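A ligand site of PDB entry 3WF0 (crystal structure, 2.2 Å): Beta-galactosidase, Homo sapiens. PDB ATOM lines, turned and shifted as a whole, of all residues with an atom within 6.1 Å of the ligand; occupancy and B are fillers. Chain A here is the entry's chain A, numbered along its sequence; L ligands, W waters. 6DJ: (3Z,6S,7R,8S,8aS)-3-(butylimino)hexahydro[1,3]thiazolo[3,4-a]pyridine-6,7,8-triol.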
ATOM      1  N   HIS A  57     -28.623  31.733 -19.986  1.00  0.00           N
ATOM      2  CA  HIS A  57     -29.002  30.428 -20.353  1.00  0.00           C
ATOM      3  C   HIS A  57     -29.991  30.513 -21.482  1.00  0.00           C
ATOM      4  O   HIS A  57     -31.129  30.927 -21.270  1.00  0.00           O
ATOM      5  CB  HIS A  57     -29.574  29.680 -19.131  1.00  0.00           C
ATOM      6  CG  HIS A  57     -28.570  29.514 -18.026  1.00  0.00           C
ATOM      7  ND1 HIS A  57     -28.927  29.191 -16.733  1.00  0.00           N
ATOM      8  CD2 HIS A  57     -27.232  29.697 -18.018  1.00  0.00           C
ATOM      9  CE1 HIS A  57     -27.838  29.140 -15.981  1.00  0.00           C
ATOM     10  NE2 HIS A  57     -26.794  29.435 -16.746  1.00  0.00           N
ATOM     11  N   TYR A  84     -24.910  27.226 -20.200  1.00  0.00           N
ATOM     12  CA  TYR A  84     -24.947  25.787 -20.060  1.00  0.00           C
ATOM     13  C   TYR A  84     -25.687  25.126 -21.219  1.00  0.00           C
ATOM     14  O   TYR A  84     -26.619  25.710 -21.779  1.00  0.00           O
ATOM     15  CB  TYR A  84     -25.720  25.394 -18.842  1.00  0.00           C
ATOM     16  CG  TYR A  84     -25.037  25.485 -17.507  1.00  0.00           C
ATOM     17  CD1 TYR A  84     -23.875  24.752 -17.211  1.00  0.00           C
ATOM     18  CD2 TYR A  84     -25.599  26.252 -16.490  1.00  0.00           C
ATOM     19  CE1 TYR A  84     -23.286  24.811 -15.946  1.00  0.00           C
ATOM     20  CE2 TYR A  84     -25.034  26.307 -15.241  1.00  0.00           C
ATOM     21  CZ  TYR A  84     -23.884  25.573 -14.959  1.00  0.00           C
ATOM     22  OH  TYR A  84     -23.354  25.669 -13.681  1.00  0.00           O
ATOM     23  N   ARG A 122     -20.414  25.591 -21.201  1.00  0.00           N
ATOM     24  CA  ARG A 122     -20.479  24.624 -20.122  1.00  0.00           C
ATOM     25  C   ARG A 122     -21.477  23.536 -20.463  1.00  0.00           C
ATOM     26  O   ARG A 122     -22.652  23.659 -20.139  1.00  0.00           O
ATOM     27  CB  ARG A 122     -20.836  25.315 -18.827  1.00  0.00           C
ATOM     28  CG  ARG A 122     -20.102  26.629 -18.650  1.00  0.00           C
ATOM     29  CD  ARG A 122     -19.847  26.939 -17.212  1.00  0.00           C
ATOM     30  NE  ARG A 122     -20.978  27.530 -16.514  1.00  0.00           N
ATOM     31  CZ  ARG A 122     -21.063  27.631 -15.194  1.00  0.00           C
ATOM     32  NH1 ARG A 122     -20.073  27.144 -14.421  1.00  0.00           N
ATOM     33  NH2 ARG A 122     -22.129  28.193 -14.622  1.00  0.00           N
ATOM     34  N   ILE A 127     -25.262  19.811 -15.236  1.00  0.00           N
ATOM     35  CA  ILE A 127     -25.050  21.268 -15.147  1.00  0.00           C
ATOM     36  C   ILE A 127     -25.542  21.893 -13.844  1.00  0.00           C
ATOM     37  O   ILE A 127     -25.187  23.015 -13.552  1.00  0.00           O
ATOM     38  CB  ILE A 127     -25.665  22.043 -16.346  1.00  0.00           C
ATOM     39  CG1 ILE A 127     -27.211  21.870 -16.356  1.00  0.00           C
ATOM     40  CG2 ILE A 127     -25.042  21.586 -17.666  1.00  0.00           C
ATOM     41  CD1 ILE A 127     -27.914  22.718 -17.397  1.00  0.00           C
ATOM     42  N   CYS A 128     -26.334  21.143 -13.067  1.00  0.00           N
ATOM     43  CA  CYS A 128     -26.934  21.665 -11.817  1.00  0.00           C
ATOM     44  C   CYS A 128     -27.962  22.769 -12.160  1.00  0.00           C
ATOM     45  O   CYS A 128     -29.073  22.453 -12.524  1.00  0.00           O
ATOM     46  CB  CYS A 128     -25.842  22.133 -10.820  1.00  0.00           C
ATOM     47  SG  CYS A 128     -26.406  22.470  -9.112  1.00  0.00           S
ATOM     48  N   ALA A 129     -27.585  24.044 -12.006  1.00  0.00           N
ATOM     49  CA  ALA A 129     -28.284  25.173 -12.634  1.00  0.00           C
ATOM     50  C   ALA A 129     -29.769  25.369 -12.256  1.00  0.00           C
ATOM     51  O   ALA A 129     -30.497  26.065 -12.988  1.00  0.00           O
ATOM     52  CB  ALA A 129     -28.130  25.093 -14.148  1.00  0.00           C
ATOM     53  N   GLU A 130     -30.205  24.756 -11.147  1.00  0.00           N
ATOM     54  CA  GLU A 130     -31.611  24.823 -10.669  1.00  0.00           C
ATOM     55  C   GLU A 130     -32.511  24.398 -11.800  1.00  0.00           C
ATOM     56  O   GLU A 130     -33.559  25.004 -12.042  1.00  0.00           O
ATOM     57  CB  GLU A 130     -32.003  26.245 -10.250  1.00  0.00           C
ATOM     58  CG  GLU A 130     -31.494  26.721  -8.915  1.00  0.00           C
ATOM     59  CD  GLU A 130     -29.984  26.977  -8.917  1.00  0.00           C
ATOM     60  OE1 GLU A 130     -29.515  28.022  -9.441  1.00  0.00           O
ATOM     61  OE2 GLU A 130     -29.262  26.135  -8.372  1.00  0.00           O
ATOM     62  N   GLN A 185     -16.168  23.991 -20.005  1.00  0.00           N
ATOM     63  CA  GLN A 185     -16.171  23.392 -18.708  1.00  0.00           C
ATOM     64  C   GLN A 185     -16.490  21.926 -18.818  1.00  0.00           C
ATOM     65  O   GLN A 185     -17.364  21.537 -19.581  1.00  0.00           O
ATOM     66  CB  GLN A 185     -17.169  24.051 -17.793  1.00  0.00           C
ATOM     67  CG  GLN A 185     -16.979  23.705 -16.304  1.00  0.00           C
ATOM     68  CD  GLN A 185     -18.038  24.375 -15.428  1.00  0.00           C
ATOM     69  OE1 GLN A 185     -17.887  25.540 -15.052  1.00  0.00           O
ATOM     70  NE2 GLN A 185     -19.136  23.655 -15.154  1.00  0.00           N
ATOM     71  N   ASN A 188     -19.539  19.802 -13.651  1.00  0.00           N
ATOM     72  CA  ASN A 188     -19.981  20.977 -12.927  1.00  0.00           C
ATOM     73  C   ASN A 188     -19.954  20.727 -11.415  1.00  0.00           C
ATOM     74  O   ASN A 188     -20.747  19.907 -10.895  1.00  0.00           O
ATOM     75  CB  ASN A 188     -21.388  21.400 -13.357  1.00  0.00           C
ATOM     76  CG  ASN A 188     -21.742  22.788 -12.847  1.00  0.00           C
ATOM     77  OD1 ASN A 188     -21.511  23.802 -13.552  1.00  0.00           O
ATOM     78  ND2 ASN A 188     -22.209  22.866 -11.581  1.00  0.00           N
ATOM     79  N   GLU A 189     -19.036  21.379 -10.707  1.00  0.00           N
ATOM     80  CA  GLU A 189     -18.831  21.148  -9.253  1.00  0.00           C
ATOM     81  C   GLU A 189     -18.802  19.690  -8.830  1.00  0.00           C
ATOM     82  O   GLU A 189     -19.414  19.301  -7.817  1.00  0.00           O
ATOM     83  CB  GLU A 189     -19.874  21.894  -8.435  1.00  0.00           C
ATOM     84  CG  GLU A 189     -19.856  23.402  -8.663  1.00  0.00           C
ATOM     85  CD  GLU A 189     -20.684  24.133  -7.609  1.00  0.00           C
ATOM     86  OE1 GLU A 189     -21.753  23.584  -7.178  1.00  0.00           O
ATOM     87  OE2 GLU A 189     -20.259  25.242  -7.202  1.00  0.00           O
ATOM     88  N   THR A 221     -15.004  23.825 -12.448  1.00  0.00           N
ATOM     89  CA  THR A 221     -15.453  24.792 -11.473  1.00  0.00           C
ATOM     90  C   THR A 221     -15.884  24.102 -10.186  1.00  0.00           C
ATOM     91  O   THR A 221     -16.560  23.080 -10.214  1.00  0.00           O
ATOM     92  CB  THR A 221     -16.654  25.577 -11.961  1.00  0.00           C
ATOM     93  OG1 THR A 221     -16.276  26.298 -13.142  1.00  0.00           O
ATOM     94  CG2 THR A 221     -17.109  26.557 -10.867  1.00  0.00           C
ATOM     95  N   ASP A 242     -15.736  29.030  -7.796  1.00  0.00           N
ATOM     96  CA  ASP A 242     -16.832  29.966  -7.714  1.00  0.00           C
ATOM     97  C   ASP A 242     -16.963  30.553  -6.297  1.00  0.00           C
ATOM     98  O   ASP A 242     -16.547  29.934  -5.316  1.00  0.00           O
ATOM     99  CB  ASP A 242     -18.153  29.366  -8.230  1.00  0.00           C
ATOM    100  CG  ASP A 242     -18.549  28.071  -7.540  1.00  0.00           C
ATOM    101  OD1 ASP A 242     -18.397  27.974  -6.318  1.00  0.00           O
ATOM    102  OD2 ASP A 242     -19.090  27.148  -8.227  1.00  0.00           O
ATOM    103  N   GLU A 269     -18.217  31.628 -11.341  1.00  0.00           N
ATOM    104  CA  GLU A 269     -19.589  31.961 -10.941  1.00  0.00           C
ATOM    105  C   GLU A 269     -19.578  32.911  -9.763  1.00  0.00           C
ATOM    106  O   GLU A 269     -19.543  32.516  -8.573  1.00  0.00           O
ATOM    107  CB  GLU A 269     -20.431  30.730 -10.608  1.00  0.00           C
ATOM    108  CG  GLU A 269     -20.403  29.573 -11.623  1.00  0.00           C
ATOM    109  CD  GLU A 269     -21.396  28.466 -11.265  1.00  0.00           C
ATOM    110  OE1 GLU A 269     -22.155  28.668 -10.287  1.00  0.00           O
ATOM    111  OE2 GLU A 269     -21.427  27.398 -11.962  1.00  0.00           O
ATOM    112  N   TYR A 271     -21.609  35.287  -7.848  1.00  0.00           N
ATOM    113  CA  TYR A 271     -23.079  35.399  -7.687  1.00  0.00           C
ATOM    114  C   TYR A 271     -23.560  36.838  -7.546  1.00  0.00           C
ATOM    115  O   TYR A 271     -23.265  37.526  -6.574  1.00  0.00           O
ATOM    116  CB  TYR A 271     -23.553  34.511  -6.504  1.00  0.00           C
ATOM    117  CG  TYR A 271     -23.073  33.090  -6.715  1.00  0.00           C
ATOM    118  CD1 TYR A 271     -23.555  32.341  -7.803  1.00  0.00           C
ATOM    119  CD2 TYR A 271     -22.115  32.519  -5.900  1.00  0.00           C
ATOM    120  CE1 TYR A 271     -23.093  31.060  -8.067  1.00  0.00           C
ATOM    121  CE2 TYR A 271     -21.656  31.210  -6.153  1.00  0.00           C
ATOM    122  CZ  TYR A 271     -22.149  30.506  -7.250  1.00  0.00           C
ATOM    123  OH  TYR A 271     -21.739  29.233  -7.531  1.00  0.00           O
ATOM    124  N   TRP A 274     -29.132  35.110  -6.066  1.00  0.00           N
ATOM    125  CA  TRP A 274     -29.316  33.741  -5.598  1.00  0.00           C
ATOM    126  C   TRP A 274     -30.641  33.133  -6.064  1.00  0.00           C
ATOM    127  O   TRP A 274     -31.499  33.840  -6.634  1.00  0.00           O
ATOM    128  CB  TRP A 274     -29.199  33.692  -4.046  1.00  0.00           C
ATOM    129  CG  TRP A 274     -28.774  32.331  -3.532  1.00  0.00           C
ATOM    130  CD1 TRP A 274     -29.442  31.542  -2.639  1.00  0.00           C
ATOM    131  CD2 TRP A 274     -27.597  31.595  -3.907  1.00  0.00           C
ATOM    132  NE1 TRP A 274     -28.764  30.387  -2.439  1.00  0.00           N
ATOM    133  CE2 TRP A 274     -27.626  30.382  -3.200  1.00  0.00           C
ATOM    134  CE3 TRP A 274     -26.519  31.844  -4.776  1.00  0.00           C
ATOM    135  CZ2 TRP A 274     -26.622  29.419  -3.306  1.00  0.00           C
ATOM    136  CZ3 TRP A 274     -25.514  30.884  -4.892  1.00  0.00           C
ATOM    137  CH2 TRP A 274     -25.583  29.680  -4.158  1.00  0.00           C
ATOM    138  N   LEU A 275     -30.819  31.840  -5.815  1.00  0.00           N
ATOM    139  CA  LEU A 275     -32.012  31.139  -6.245  1.00  0.00           C
ATOM    140  C   LEU A 275     -33.100  31.271  -5.188  1.00  0.00           C
ATOM    141  O   LEU A 275     -32.792  31.612  -4.029  1.00  0.00           O
ATOM    142  CB  LEU A 275     -31.664  29.655  -6.489  1.00  0.00           C
ATOM    143  CG  LEU A 275     -31.032  28.960  -5.271  1.00  0.00           C
ATOM    144  CD1 LEU A 275     -32.026  27.917  -4.807  1.00  0.00           C
ATOM    145  CD2 LEU A 275     -29.688  28.308  -5.589  1.00  0.00           C
ATOM    146  N   TYR A 307     -22.880  35.301 -12.390  1.00  0.00           N
ATOM    147  CA  TYR A 307     -23.964  34.316 -12.414  1.00  0.00           C
ATOM    148  C   TYR A 307     -25.118  34.822 -11.545  1.00  0.00           C
ATOM    149  O   TYR A 307     -24.938  34.933 -10.367  1.00  0.00           O
ATOM    150  CB  TYR A 307     -23.456  32.943 -11.857  1.00  0.00           C
ATOM    151  CG  TYR A 307     -24.418  31.797 -12.072  1.00  0.00           C
ATOM    152  CD1 TYR A 307     -25.600  31.693 -11.312  1.00  0.00           C
ATOM    153  CD2 TYR A 307     -24.182  30.850 -13.067  1.00  0.00           C
ATOM    154  CE1 TYR A 307     -26.505  30.635 -11.520  1.00  0.00           C
ATOM    155  CE2 TYR A 307     -25.075  29.796 -13.271  1.00  0.00           C
ATOM    156  CZ  TYR A 307     -26.231  29.700 -12.504  1.00  0.00           C
ATOM    157  OH  TYR A 307     -27.127  28.682 -12.762  1.00  0.00           O
ATOM    158  N   TYR A 332     -36.839  32.547 -12.954  1.00  0.00           N
ATOM    159  CA  TYR A 332     -35.416  32.438 -12.663  1.00  0.00           C
ATOM    160  C   TYR A 332     -34.783  33.859 -12.683  1.00  0.00           C
ATOM    161  O   TYR A 332     -33.600  34.041 -13.001  1.00  0.00           O
ATOM    162  CB  TYR A 332     -34.715  31.481 -13.654  1.00  0.00           C
ATOM    163  CG  TYR A 332     -33.375  30.926 -13.140  1.00  0.00           C
ATOM    164  CD1 TYR A 332     -33.323  30.148 -11.967  1.00  0.00           C
ATOM    165  CD2 TYR A 332     -32.160  31.208 -13.794  1.00  0.00           C
ATOM    166  CE1 TYR A 332     -32.107  29.657 -11.486  1.00  0.00           C
ATOM    167  CE2 TYR A 332     -30.957  30.692 -13.323  1.00  0.00           C
ATOM    168  CZ  TYR A 332     -30.932  29.925 -12.173  1.00  0.00           C
ATOM    169  OH  TYR A 332     -29.738  29.416 -11.680  1.00  0.00           O
ATOM    170  N   TYR A 334     -33.585  35.621 -10.389  1.00  0.00           N
ATOM    171  CA  TYR A 334     -32.297  35.455  -9.714  1.00  0.00           C
ATOM    172  C   TYR A 334     -31.775  36.799  -9.213  1.00  0.00           C
ATOM    173  O   TYR A 334     -30.623  36.911  -8.812  1.00  0.00           O
ATOM    174  CB  TYR A 334     -31.257  34.767 -10.641  1.00  0.00           C
ATOM    175  CG  TYR A 334     -30.433  33.664  -9.993  1.00  0.00           C
ATOM    176  CD1 TYR A 334     -30.999  32.422  -9.743  1.00  0.00           C
ATOM    177  CD2 TYR A 334     -29.063  33.849  -9.659  1.00  0.00           C
ATOM    178  CE1 TYR A 334     -30.255  31.381  -9.206  1.00  0.00           C
ATOM    179  CE2 TYR A 334     -28.304  32.795  -9.080  1.00  0.00           C
ATOM    180  CZ  TYR A 334     -28.917  31.571  -8.843  1.00  0.00           C
ATOM    181  OH  TYR A 334     -28.221  30.503  -8.270  1.00  0.00           O
ATOM    182  N   ASN A 485     -31.720  18.714  -8.498  1.00  0.00           N
ATOM    183  CA  ASN A 485     -30.616  19.058  -9.396  1.00  0.00           C
ATOM    184  C   ASN A 485     -29.240  19.109  -8.688  1.00  0.00           C
ATOM    185  O   ASN A 485     -28.230  19.362  -9.312  1.00  0.00           O
ATOM    186  CB  ASN A 485     -30.921  20.387 -10.092  1.00  0.00           C
ATOM    187  CG  ASN A 485     -30.998  21.556  -9.135  1.00  0.00           C
ATOM    188  OD1 ASN A 485     -29.969  22.133  -8.753  1.00  0.00           O
ATOM    189  ND2 ASN A 485     -32.205  21.949  -8.761  1.00  0.00           N
ATOM    190  N   TYR A 486     -29.216  18.851  -7.381  1.00  0.00           N
ATOM    191  CA  TYR A 486     -27.985  18.971  -6.580  1.00  0.00           C
ATOM    192  C   TYR A 486     -28.073  18.026  -5.411  1.00  0.00           C
ATOM    193  O   TYR A 486     -29.096  17.969  -4.725  1.00  0.00           O
ATOM    194  CB  TYR A 486     -27.786  20.389  -6.037  1.00  0.00           C
ATOM    195  CG  TYR A 486     -26.481  20.610  -5.222  1.00  0.00           C
ATOM    196  CD1 TYR A 486     -25.230  20.720  -5.850  1.00  0.00           C
ATOM    197  CD2 TYR A 486     -26.523  20.711  -3.809  1.00  0.00           C
ATOM    198  CE1 TYR A 486     -24.061  20.938  -5.124  1.00  0.00           C
ATOM    199  CE2 TYR A 486     -25.368  20.900  -3.051  1.00  0.00           C
ATOM    200  CZ  TYR A 486     -24.134  21.020  -3.712  1.00  0.00           C
ATOM    201  OH  TYR A 486     -22.981  21.207  -2.977  1.00  0.00           O
HETATM  202  O2  6DJ L   1     -22.646  25.468 -10.644  1.00  0.00           O
HETATM  203  C2  6DJ L   1     -23.822  25.619  -9.842  1.00  0.00           C
HETATM  204  C3  6DJ L   1     -24.853  26.467 -10.600  1.00  0.00           C
HETATM  205  O3  6DJ L   1     -25.319  25.661 -11.715  1.00  0.00           O
HETATM  206  C1  6DJ L   1     -23.381  26.269  -8.526  1.00  0.00           C
HETATM  207  N5  6DJ L   1     -24.595  26.566  -7.800  1.00  0.00           N
HETATM  208  C5  6DJ L   1     -25.370  27.634  -8.420  1.00  0.00           C
HETATM  209  C4  6DJ L   1     -25.961  26.975  -9.679  1.00  0.00           C
HETATM  210  O4  6DJ L   1     -26.765  25.866  -9.257  1.00  0.00           O
HETATM  211  S6  6DJ L   1     -26.551  26.679  -6.135  1.00  0.00           S
HETATM  212  C6  6DJ L   1     -26.404  27.982  -7.346  1.00  0.00           C
HETATM  213  C7  6DJ L   1     -25.088  26.014  -6.682  1.00  0.00           C
HETATM  214  N8  6DJ L   1     -24.460  25.076  -6.110  1.00  0.00           N
HETATM  215  C9  6DJ L   1     -24.779  24.363  -4.874  1.00  0.00           C
HETATM  216  C10 6DJ L   1     -24.044  25.168  -3.765  1.00  0.00           C
HETATM  217  C11 6DJ L   1     -24.400  24.672  -2.347  1.00  0.00           C
HETATM  218  C12 6DJ L   1     -24.353  25.756  -1.279  1.00  0.00           C
HETATM  219  O   HOH W   1     -22.086  27.353  -5.498  1.00  0.00           O
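OE2 of Glu 269 is in hydrogen-bond range of O2 of the ligand. The side-chain carboxylate (OE2) of Glu 130 sits at hydrogen-bond distance from an oxygen (O4) of the ligand, at 2.7 Å. OH of Tyr 84 is in hydrogen-bond range of O3 of the ligand (2.8 Å). O3 of the ligand sits at hydrogen-bond distance from N of Ala 129 (2.8 Å). An oxygen (O2) of the ligand is in hydrogen-bond range of the side-chain amide nitrogen of Asn 188, at 2.8 Å. O of Ile 127 is in hydrogen-bond range of O3 of the ligand (3.2 Å). The side-chain sulfur (SG) of Cys 128 is in hydrogen-bond range of an oxygen (O4) of the ligand (3.4 Å).
The side-chain carboxylate of Glu 269 is in hydrogen-bond range of the side-chain hydroxyl of Tyr 84 (3.1 Å). OE2 of Glu 269 is in salt-bridge range of NH1 of Arg 122, 2.8 Å away. The side-chain carboxylate (OE1) of Glu 130 sits at hydrogen-bond distance from the side-chain hydroxyl (OH) of Tyr 334, at 3.0 Å. OH of Tyr 332 lies within hydrogen-bond range of OE1 of Glu 130 (2.6 Å). OH of Tyr 84 sits at hydrogen-bond distance from OD1 of Asn 188 (2.6 Å). The side-chain hydroxyl of Tyr 84 sits close to the backbone carbonyl oxygen of Ile 127 (3.2 Å). O of Thr 221 lies within hydrogen-bond range of N of Glu 189. The side-chain carboxylate (OD2) of Asp 242 sits close to the side-chain hydroxyl (OH) of Tyr 271 (3.4 Å).
N8 of the ligand lies close to OE1 of Glu 189. Residues that only touch the ligand: Tyr 334, Tyr 486, Tyr 271, Leu 275, Tyr 307 and Trp 274. Hydrophobic or aromatic side chains within 4 Å of the ligand: Tyr 84, Ala 129, Trp 274, Leu 275, Tyr 307 and Tyr 486. 14 residues have an atom within 4 Å of the ligand: Tyr 84, Ile 127, Cys 128, Ala 129, Glu 130, Asn 188, Glu 189, Glu 269, Tyr 271, Trp 274, Leu 275, Tyr 307, Tyr 334 and Tyr 486. The nearest printed residue that does not touch the ligand is Asp 242 (4.4 Å).
Water W1 lies within hydrogen-bond range of OH of Tyr 271, OE2 of Glu 189 and N8 of the ligand.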
